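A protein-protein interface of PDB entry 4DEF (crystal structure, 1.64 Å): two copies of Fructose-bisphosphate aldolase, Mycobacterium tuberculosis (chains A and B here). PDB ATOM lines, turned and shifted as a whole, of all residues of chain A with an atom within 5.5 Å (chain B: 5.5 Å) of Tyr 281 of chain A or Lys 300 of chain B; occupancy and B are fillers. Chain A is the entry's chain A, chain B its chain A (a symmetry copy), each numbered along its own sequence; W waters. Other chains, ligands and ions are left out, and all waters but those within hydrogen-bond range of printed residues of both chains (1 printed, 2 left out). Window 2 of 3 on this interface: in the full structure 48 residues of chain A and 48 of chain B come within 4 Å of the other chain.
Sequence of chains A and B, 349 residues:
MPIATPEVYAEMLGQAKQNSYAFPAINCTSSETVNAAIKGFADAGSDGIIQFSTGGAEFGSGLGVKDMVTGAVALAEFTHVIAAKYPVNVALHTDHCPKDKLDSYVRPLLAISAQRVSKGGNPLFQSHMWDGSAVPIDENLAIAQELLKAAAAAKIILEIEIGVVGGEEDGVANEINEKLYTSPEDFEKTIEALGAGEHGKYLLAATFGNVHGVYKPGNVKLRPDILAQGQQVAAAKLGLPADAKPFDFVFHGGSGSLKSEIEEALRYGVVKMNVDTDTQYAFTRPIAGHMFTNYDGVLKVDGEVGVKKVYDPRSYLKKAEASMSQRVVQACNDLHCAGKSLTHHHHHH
The backbone NH (N) of Lys 300 of chain B sits at hydrogen-bond distance from the side-chain hydroxyl (OH) of Tyr 281 of chain A.
O of Tyr 311 of chain B sits at hydrogen-bond distance from OG1 of Thr 284 of chain A (2.6 Å).
OD1 of Asp 276 of chain A lies close to OE1 of Gln 280 of chain A (3.2 Å).
OG1 of Thr 284 of chain A lies within hydrogen-bond range of O of Gln 280 of chain A (3.2 Å).
CG2 of Thr 277 of chain A touches OH of Tyr 311 of chain B, at 3.1 Å.
Tyr 311 of chain B touches Gln 280 of chain A.
CE1 of Tyr 281 of chain A touches O of Val 298 of chain B (3.4 Å).
Leu 299 of chain B touches Tyr 281 of chain A (CA to OH, 3.7 Å).
Tyr 281 of chain A touches Tyr 311 of chain B.
CD of Arg 285 of chain A touches CD2 of Leu 299 of chain B, 3.6 Å away.
Tyr 281 of chain A touches just these residues of chain B: Val 298, Leu 299, Lys 300 and Tyr 311.
Lys 300 of chain B touches just one residue of chain A: Tyr 281.
Printed residues of chain B within 4 Å of Gln 280 of chain A: Tyr 311.
Of the printed residues of chain B, Arg 285 of chain A touches Leu 299.
Printed residues of chain B within 4 Å of Thr 277 of chain A: Tyr 311 (3.1 Å).
Printed residues of chain B within 4 Å of Thr 284 of chain A: Tyr 311 (2.6 Å).
Printed residues of chain A within 4 Å of Leu 299 of chain B: Tyr 281 (3.7 Å) and Arg 285 (3.6 Å).
Phe 283 of chain A touches none of the printed residues of chain B.
Gly 306 of chain B touches none of the printed residues of chain A.
The nearest residue of chain B that does not touch Tyr 281 of chain A is Gly 297 of chain B (5.1 Å).
The nearest residue of chain A that does not touch Lys 300 of chain B is Asp 278 of chain A (5.4 Å).
The nearest printed residue of chain B that does not touch Thr 277 of chain A is Val 305 of chain B (7.1 Å).
Of the 11 printed residues of chain A, 5 touch a printed residue of chain B.
Hydrophobic or aromatic side chains of chain A within 4 Å of the printed part of chain B: Tyr 281.
Along chain A the printed residues that touch a printed residue of chain B span positions 277 to 285.
Of the 11 printed residues of chain B, 4 touch a printed residue of chain A.
Along chain B the printed residues that touch a printed residue of chain A span positions 298 to 311.
Among the printed residues, 8 pairs touch across the chains.
Among the printed residues, no Asp or Glu carboxylate lies within 4 Å of a Lys or Arg side-chain nitrogen of the other chain.
No position is printed for both chains.
Of the 8 pairs that touch across the chains among the printed residues, none has its exchanged pair printed and touching as well.
Water W1 lies within hydrogen-bond range of O of Val 298 of chain B (2.7 Å), N of Arg 285 of chain A (3.2 Å) and O of Tyr 281 of chain A (3.3 Å).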
ATOM      1  N   ASP A 276       0.682  21.802   4.411  1.00  0.00           N
ATOM      2  CA  ASP A 276      -0.111  21.446   3.249  1.00  0.00           C
ATOM      3  C   ASP A 276       0.814  20.987   2.139  1.00  0.00           C
ATOM      4  O   ASP A 276       0.750  19.835   1.729  1.00  0.00           O
ATOM      5  CB  ASP A 276      -0.981  22.629   2.800  1.00  0.00           C
ATOM      6  CG  ASP A 276      -2.025  22.242   1.768  1.00  0.00           C
ATOM      7  OD1 ASP A 276      -2.249  21.031   1.535  1.00  0.00           O
ATOM      8  OD2 ASP A 276      -2.658  23.164   1.197  1.00  0.00           O
ATOM      9  N   THR A 277       1.707  21.865   1.680  1.00  0.00           N
ATOM     10  CA  THR A 277       2.591  21.564   0.555  1.00  0.00           C
ATOM     11  C   THR A 277       3.361  20.257   0.756  1.00  0.00           C
ATOM     12  O   THR A 277       3.445  19.419  -0.144  1.00  0.00           O
ATOM     13  CB  THR A 277       3.586  22.722   0.323  1.00  0.00           C
ATOM     14  OG1 THR A 277       2.855  23.927   0.087  1.00  0.00           O
ATOM     15  CG2 THR A 277       4.480  22.445  -0.876  1.00  0.00           C
ATOM     16  N   ASP A 278       3.936  20.111   1.949  1.00  0.00           N
ATOM     17  CA  ASP A 278       4.783  18.956   2.245  1.00  0.00           C
ATOM     18  C   ASP A 278       4.013  17.636   2.295  1.00  0.00           C
ATOM     19  O   ASP A 278       4.527  16.588   1.859  1.00  0.00           O
ATOM     20  CB  ASP A 278       5.594  19.177   3.518  1.00  0.00           C
ATOM     21  CG  ASP A 278       6.831  20.060   3.276  1.00  0.00           C
ATOM     22  OD1 ASP A 278       7.092  20.452   2.112  1.00  0.00           O
ATOM     23  OD2 ASP A 278       7.538  20.350   4.256  1.00  0.00           O
ATOM     24  N   THR A 279       2.789  17.686   2.808  1.00  0.00           N
ATOM     25  CA  THR A 279       1.948  16.477   2.832  1.00  0.00           C
ATOM     26  C   THR A 279       1.355  16.176   1.454  1.00  0.00           C
ATOM     27  O   THR A 279       1.118  15.005   1.132  1.00  0.00           O
ATOM     28  CB  THR A 279       0.858  16.498   3.934  1.00  0.00           C
ATOM     29  OG1 THR A 279       0.311  17.822   4.062  1.00  0.00           O
ATOM     30  CG2 THR A 279       1.470  16.126   5.255  1.00  0.00           C
ATOM     31  N   GLN A 280       1.103  17.214   0.652  1.00  0.00           N
ATOM     32  CA  GLN A 280       0.698  17.004  -0.749  1.00  0.00           C
ATOM     33  C   GLN A 280       1.791  16.243  -1.508  1.00  0.00           C
ATOM     34  O   GLN A 280       1.501  15.256  -2.211  1.00  0.00           O
ATOM     35  CB  GLN A 280       0.410  18.338  -1.462  1.00  0.00           C
ATOM     36  CG  GLN A 280      -0.835  19.093  -0.978  1.00  0.00           C
ATOM     37  CD  GLN A 280      -1.091  20.380  -1.769  1.00  0.00           C
ATOM     38  OE1 GLN A 280      -2.164  20.984  -1.680  1.00  0.00           O
ATOM     39  NE2 GLN A 280      -0.121  20.787  -2.549  1.00  0.00           N
ATOM     40  N   TYR A 281       3.045  16.673  -1.364  1.00  0.00           N
ATOM     41  CA  TYR A 281       4.132  15.989  -2.081  1.00  0.00           C
ATOM     42  C   TYR A 281       4.225  14.533  -1.626  1.00  0.00           C
ATOM     43  O   TYR A 281       4.354  13.630  -2.454  1.00  0.00           O
ATOM     44  CB  TYR A 281       5.489  16.696  -1.929  1.00  0.00           C
ATOM     45  CG  TYR A 281       6.530  16.047  -2.811  1.00  0.00           C
ATOM     46  CD1 TYR A 281       6.577  16.324  -4.180  1.00  0.00           C
ATOM     47  CD2 TYR A 281       7.427  15.108  -2.293  1.00  0.00           C
ATOM     48  CE1 TYR A 281       7.494  15.705  -5.012  1.00  0.00           C
ATOM     49  CE2 TYR A 281       8.362  14.482  -3.121  1.00  0.00           C
ATOM     50  CZ  TYR A 281       8.387  14.778  -4.471  1.00  0.00           C
ATOM     51  OH  TYR A 281       9.316  14.167  -5.289  1.00  0.00           O
ATOM     52  N   ALA A 282       4.143  14.332  -0.315  1.00  0.00           N
ATOM     53  CA  ALA A 282       4.206  12.983   0.265  1.00  0.00           C
ATOM     54  C   ALA A 282       3.075  12.087  -0.235  1.00  0.00           C
ATOM     55  O   ALA A 282       3.291  10.895  -0.474  1.00  0.00           O
ATOM     56  CB  ALA A 282       4.192  13.054   1.791  1.00  0.00           C
ATOM     57  N   PHE A 283       1.879  12.645  -0.389  1.00  0.00           N
ATOM     58  CA  PHE A 283       0.740  11.866  -0.867  1.00  0.00           C
ATOM     59  C   PHE A 283       0.924  11.497  -2.347  1.00  0.00           C
ATOM     60  O   PHE A 283       0.732  10.351  -2.748  1.00  0.00           O
ATOM     61  CB  PHE A 283      -0.546  12.675  -0.676  1.00  0.00           C
ATOM     62  CG  PHE A 283      -1.800  11.901  -0.946  1.00  0.00           C
ATOM     63  CD1 PHE A 283      -2.417  11.172   0.080  1.00  0.00           C
ATOM     64  CD2 PHE A 283      -2.386  11.908  -2.214  1.00  0.00           C
ATOM     65  CE1 PHE A 283      -3.584  10.457  -0.163  1.00  0.00           C
ATOM     66  CE2 PHE A 283      -3.557  11.201  -2.456  1.00  0.00           C
ATOM     67  CZ  PHE A 283      -4.165  10.487  -1.426  1.00  0.00           C
ATOM     68  N   THR A 284       1.327  12.467  -3.160  1.00  0.00           N
ATOM     69  CA  THR A 284       1.431  12.247  -4.594  1.00  0.00           C
ATOM     70  C   THR A 284       2.616  11.367  -5.011  1.00  0.00           C
ATOM     71  O   THR A 284       2.519  10.626  -5.989  1.00  0.00           O
ATOM     72  CB  THR A 284       1.454  13.593  -5.330  1.00  0.00           C
ATOM     73  OG1 THR A 284       0.222  14.265  -5.027  1.00  0.00           O
ATOM     74  CG2 THR A 284       1.609  13.404  -6.857  1.00  0.00           C
ATOM     75  N   ARG A 285       3.713  11.429  -4.253  1.00  0.00           N
ATOM     76  CA  ARG A 285       4.970  10.826  -4.698  1.00  0.00           C
ATOM     77  C   ARG A 285       4.878   9.320  -5.025  1.00  0.00           C
ATOM     78  O   ARG A 285       5.343   8.909  -6.097  1.00  0.00           O
ATOM     79  CB  ARG A 285       6.090  11.135  -3.700  1.00  0.00           C
ATOM     80  CG  ARG A 285       7.409  10.454  -4.012  1.00  0.00           C
ATOM     81  CD  ARG A 285       8.036  10.924  -5.310  1.00  0.00           C
ATOM     82  NE  ARG A 285       9.285  10.194  -5.543  1.00  0.00           N
ATOM     83  CZ  ARG A 285       9.361   8.995  -6.123  1.00  0.00           C
ATOM     84  NH1 ARG A 285       8.273   8.377  -6.565  1.00  0.00           N
ATOM     85  NH2 ARG A 285      10.550   8.412  -6.278  1.00  0.00           N
ATOM     86  N   PRO A 286       4.243   8.514  -4.146  1.00  0.00           N
ATOM     87  CA  PRO A 286       4.116   7.099  -4.515  1.00  0.00           C
ATOM     88  C   PRO A 286       3.091   6.787  -5.579  1.00  0.00           C
ATOM     89  O   PRO A 286       3.148   5.703  -6.192  1.00  0.00           O
ATOM     90  CB  PRO A 286       3.756   6.392  -3.195  1.00  0.00           C
ATOM     91  CG  PRO A 286       3.279   7.452  -2.270  1.00  0.00           C
ATOM     92  CD  PRO A 286       3.718   8.794  -2.792  1.00  0.00           C
ATOM     93  N   GLY B 297       7.220  17.770 -12.488  1.00  0.00           N
ATOM     94  CA  GLY B 297       6.490  18.584 -11.516  1.00  0.00           C
ATOM     95  C   GLY B 297       6.046  17.735 -10.337  1.00  0.00           C
ATOM     96  O   GLY B 297       6.090  18.178  -9.187  1.00  0.00           O
ATOM     97  N   VAL B 298       5.624  16.505 -10.615  1.00  0.00           N
ATOM     98  CA  VAL B 298       5.224  15.576  -9.545  1.00  0.00           C
ATOM     99  C   VAL B 298       6.412  14.874  -8.904  1.00  0.00           C
ATOM    100  O   VAL B 298       6.279  14.264  -7.824  1.00  0.00           O
ATOM    101  CB  VAL B 298       4.169  14.519  -9.996  1.00  0.00           C
ATOM    102  CG1 VAL B 298       2.907  15.215 -10.517  1.00  0.00           C
ATOM    103  CG2 VAL B 298       4.745  13.554 -11.025  1.00  0.00           C
ATOM    104  N   LEU B 299       7.571  14.946  -9.555  1.00  0.00           N
ATOM    105  CA  LEU B 299       8.812  14.459  -8.944  1.00  0.00           C
ATOM    106  C   LEU B 299       9.779  15.609  -8.799  1.00  0.00           C
ATOM    107  O   LEU B 299       9.799  16.519  -9.642  1.00  0.00           O
ATOM    108  CB  LEU B 299       9.475  13.371  -9.789  1.00  0.00           C
ATOM    109  CG  LEU B 299       8.675  12.126 -10.174  1.00  0.00           C
ATOM    110  CD1 LEU B 299       9.488  11.258 -11.139  1.00  0.00           C
ATOM    111  CD2 LEU B 299       8.282  11.377  -8.894  1.00  0.00           C
ATOM    112  N   LYS B 300      10.562  15.578  -7.728  1.00  0.00           N
ATOM    113  CA  LYS B 300      11.669  16.527  -7.563  1.00  0.00           C
ATOM    114  C   LYS B 300      12.863  15.973  -8.331  1.00  0.00           C
ATOM    115  O   LYS B 300      13.497  15.015  -7.890  1.00  0.00           O
ATOM    116  CB  LYS B 300      11.981  16.717  -6.078  1.00  0.00           C
ATOM    117  CG  LYS B 300      10.821  17.322  -5.315  1.00  0.00           C
ATOM    118  CD  LYS B 300      11.174  17.551  -3.853  1.00  0.00           C
ATOM    119  CE  LYS B 300       9.953  17.924  -3.047  1.00  0.00           C
ATOM    120  NZ  LYS B 300      10.329  18.142  -1.614  1.00  0.00           N
ATOM    121  N   VAL B 301      13.127  16.541  -9.502  1.00  0.00           N
ATOM    122  CA  VAL B 301      14.151  16.007 -10.394  1.00  0.00           C
ATOM    123  C   VAL B 301      15.342  16.953 -10.514  1.00  0.00           C
ATOM    124  O   VAL B 301      15.181  18.171 -10.514  1.00  0.00           O
ATOM    125  CB  VAL B 301      13.567  15.692 -11.787  1.00  0.00           C
ATOM    126  CG1 VAL B 301      13.087  16.965 -12.469  1.00  0.00           C
ATOM    127  CG2 VAL B 301      14.568  14.933 -12.651  1.00  0.00           C
ATOM    128  N   ASP B 302      16.534  16.367 -10.599  1.00  0.00           N
ATOM    129  CA  ASP B 302      17.793  17.100 -10.892  1.00  0.00           C
ATOM    130  C   ASP B 302      18.028  18.284  -9.951  1.00  0.00           C
ATOM    131  O   ASP B 302      18.509  19.341 -10.367  1.00  0.00           O
ATOM    132  CB  ASP B 302      17.845  17.558 -12.361  1.00  0.00           C
ATOM    133  CG  ASP B 302      17.956  16.394 -13.343  1.00  0.00           C
ATOM    134  OD1 ASP B 302      18.531  15.354 -13.000  1.00  0.00           O
ATOM    135  OD2 ASP B 302      17.459  16.526 -14.470  1.00  0.00           O
ATOM    136  N   GLY B 303      17.656  18.098  -8.693  1.00  0.00           N
ATOM    137  CA  GLY B 303      17.861  19.125  -7.672  1.00  0.00           C
ATOM    138  C   GLY B 303      16.780  20.185  -7.604  1.00  0.00           C
ATOM    139  O   GLY B 303      16.851  21.076  -6.749  1.00  0.00           O
ATOM    140  N   GLU B 304      15.778  20.086  -8.480  1.00  0.00           N
ATOM    141  CA  GLU B 304      14.634  21.004  -8.477  1.00  0.00           C
ATOM    142  C   GLU B 304      13.610  20.573  -7.420  1.00  0.00           C
ATOM    143  O   GLU B 304      13.730  19.495  -6.827  1.00  0.00           O
ATOM    144  CB  GLU B 304      13.988  21.125  -9.866  1.00  0.00           C
ATOM    145  CG  GLU B 304      14.938  21.505 -11.009  1.00  0.00           C
ATOM    146  CD  GLU B 304      15.401  22.960 -11.001  1.00  0.00           C
ATOM    147  OE1 GLU B 304      14.785  23.808 -10.326  1.00  0.00           O
ATOM    148  OE2 GLU B 304      16.403  23.266 -11.689  1.00  0.00           O
ATOM    149  N   VAL B 305      12.618  21.418  -7.163  1.00  0.00           N
ATOM    150  CA  VAL B 305      11.693  21.161  -6.060  1.00  0.00           C
ATOM    151  C   VAL B 305      10.286  20.784  -6.503  1.00  0.00           C
ATOM    152  O   VAL B 305       9.364  20.802  -5.694  1.00  0.00           O
ATOM    153  CB  VAL B 305      11.621  22.355  -5.082  1.00  0.00           C
ATOM    154  CG1 VAL B 305      12.995  22.646  -4.504  1.00  0.00           C
ATOM    155  CG2 VAL B 305      11.043  23.587  -5.769  1.00  0.00           C
ATOM    156  N   GLY B 306      10.128  20.424  -7.775  1.00  0.00           N
ATOM    157  CA  GLY B 306       8.806  20.045  -8.306  1.00  0.00           C
ATOM    158  C   GLY B 306       7.910  21.255  -8.474  1.00  0.00           C
ATOM    159  O   GLY B 306       8.364  22.400  -8.336  1.00  0.00           O
ATOM    160  N   TYR B 311       1.491  18.660  -8.147  1.00  0.00           N
ATOM    161  CA  TYR B 311       1.480  17.610  -7.119  1.00  0.00           C
ATOM    162  C   TYR B 311       0.392  17.756  -6.053  1.00  0.00           C
ATOM    163  O   TYR B 311       0.194  16.857  -5.231  1.00  0.00           O
ATOM    164  CB  TYR B 311       2.878  17.268  -6.547  1.00  0.00           C
ATOM    165  CG  TYR B 311       3.597  18.314  -5.708  1.00  0.00           C
ATOM    166  CD1 TYR B 311       3.153  18.643  -4.424  1.00  0.00           C
ATOM    167  CD2 TYR B 311       4.777  18.910  -6.169  1.00  0.00           C
ATOM    168  CE1 TYR B 311       3.840  19.560  -3.640  1.00  0.00           C
ATOM    169  CE2 TYR B 311       5.467  19.834  -5.395  1.00  0.00           C
ATOM    170  CZ  TYR B 311       4.996  20.151  -4.135  1.00  0.00           C
ATOM    171  OH  TYR B 311       5.687  21.065  -3.371  1.00  0.00           O
HETATM  172  O   HOH W   1       4.693  14.066  -5.680  1.00  0.00           O
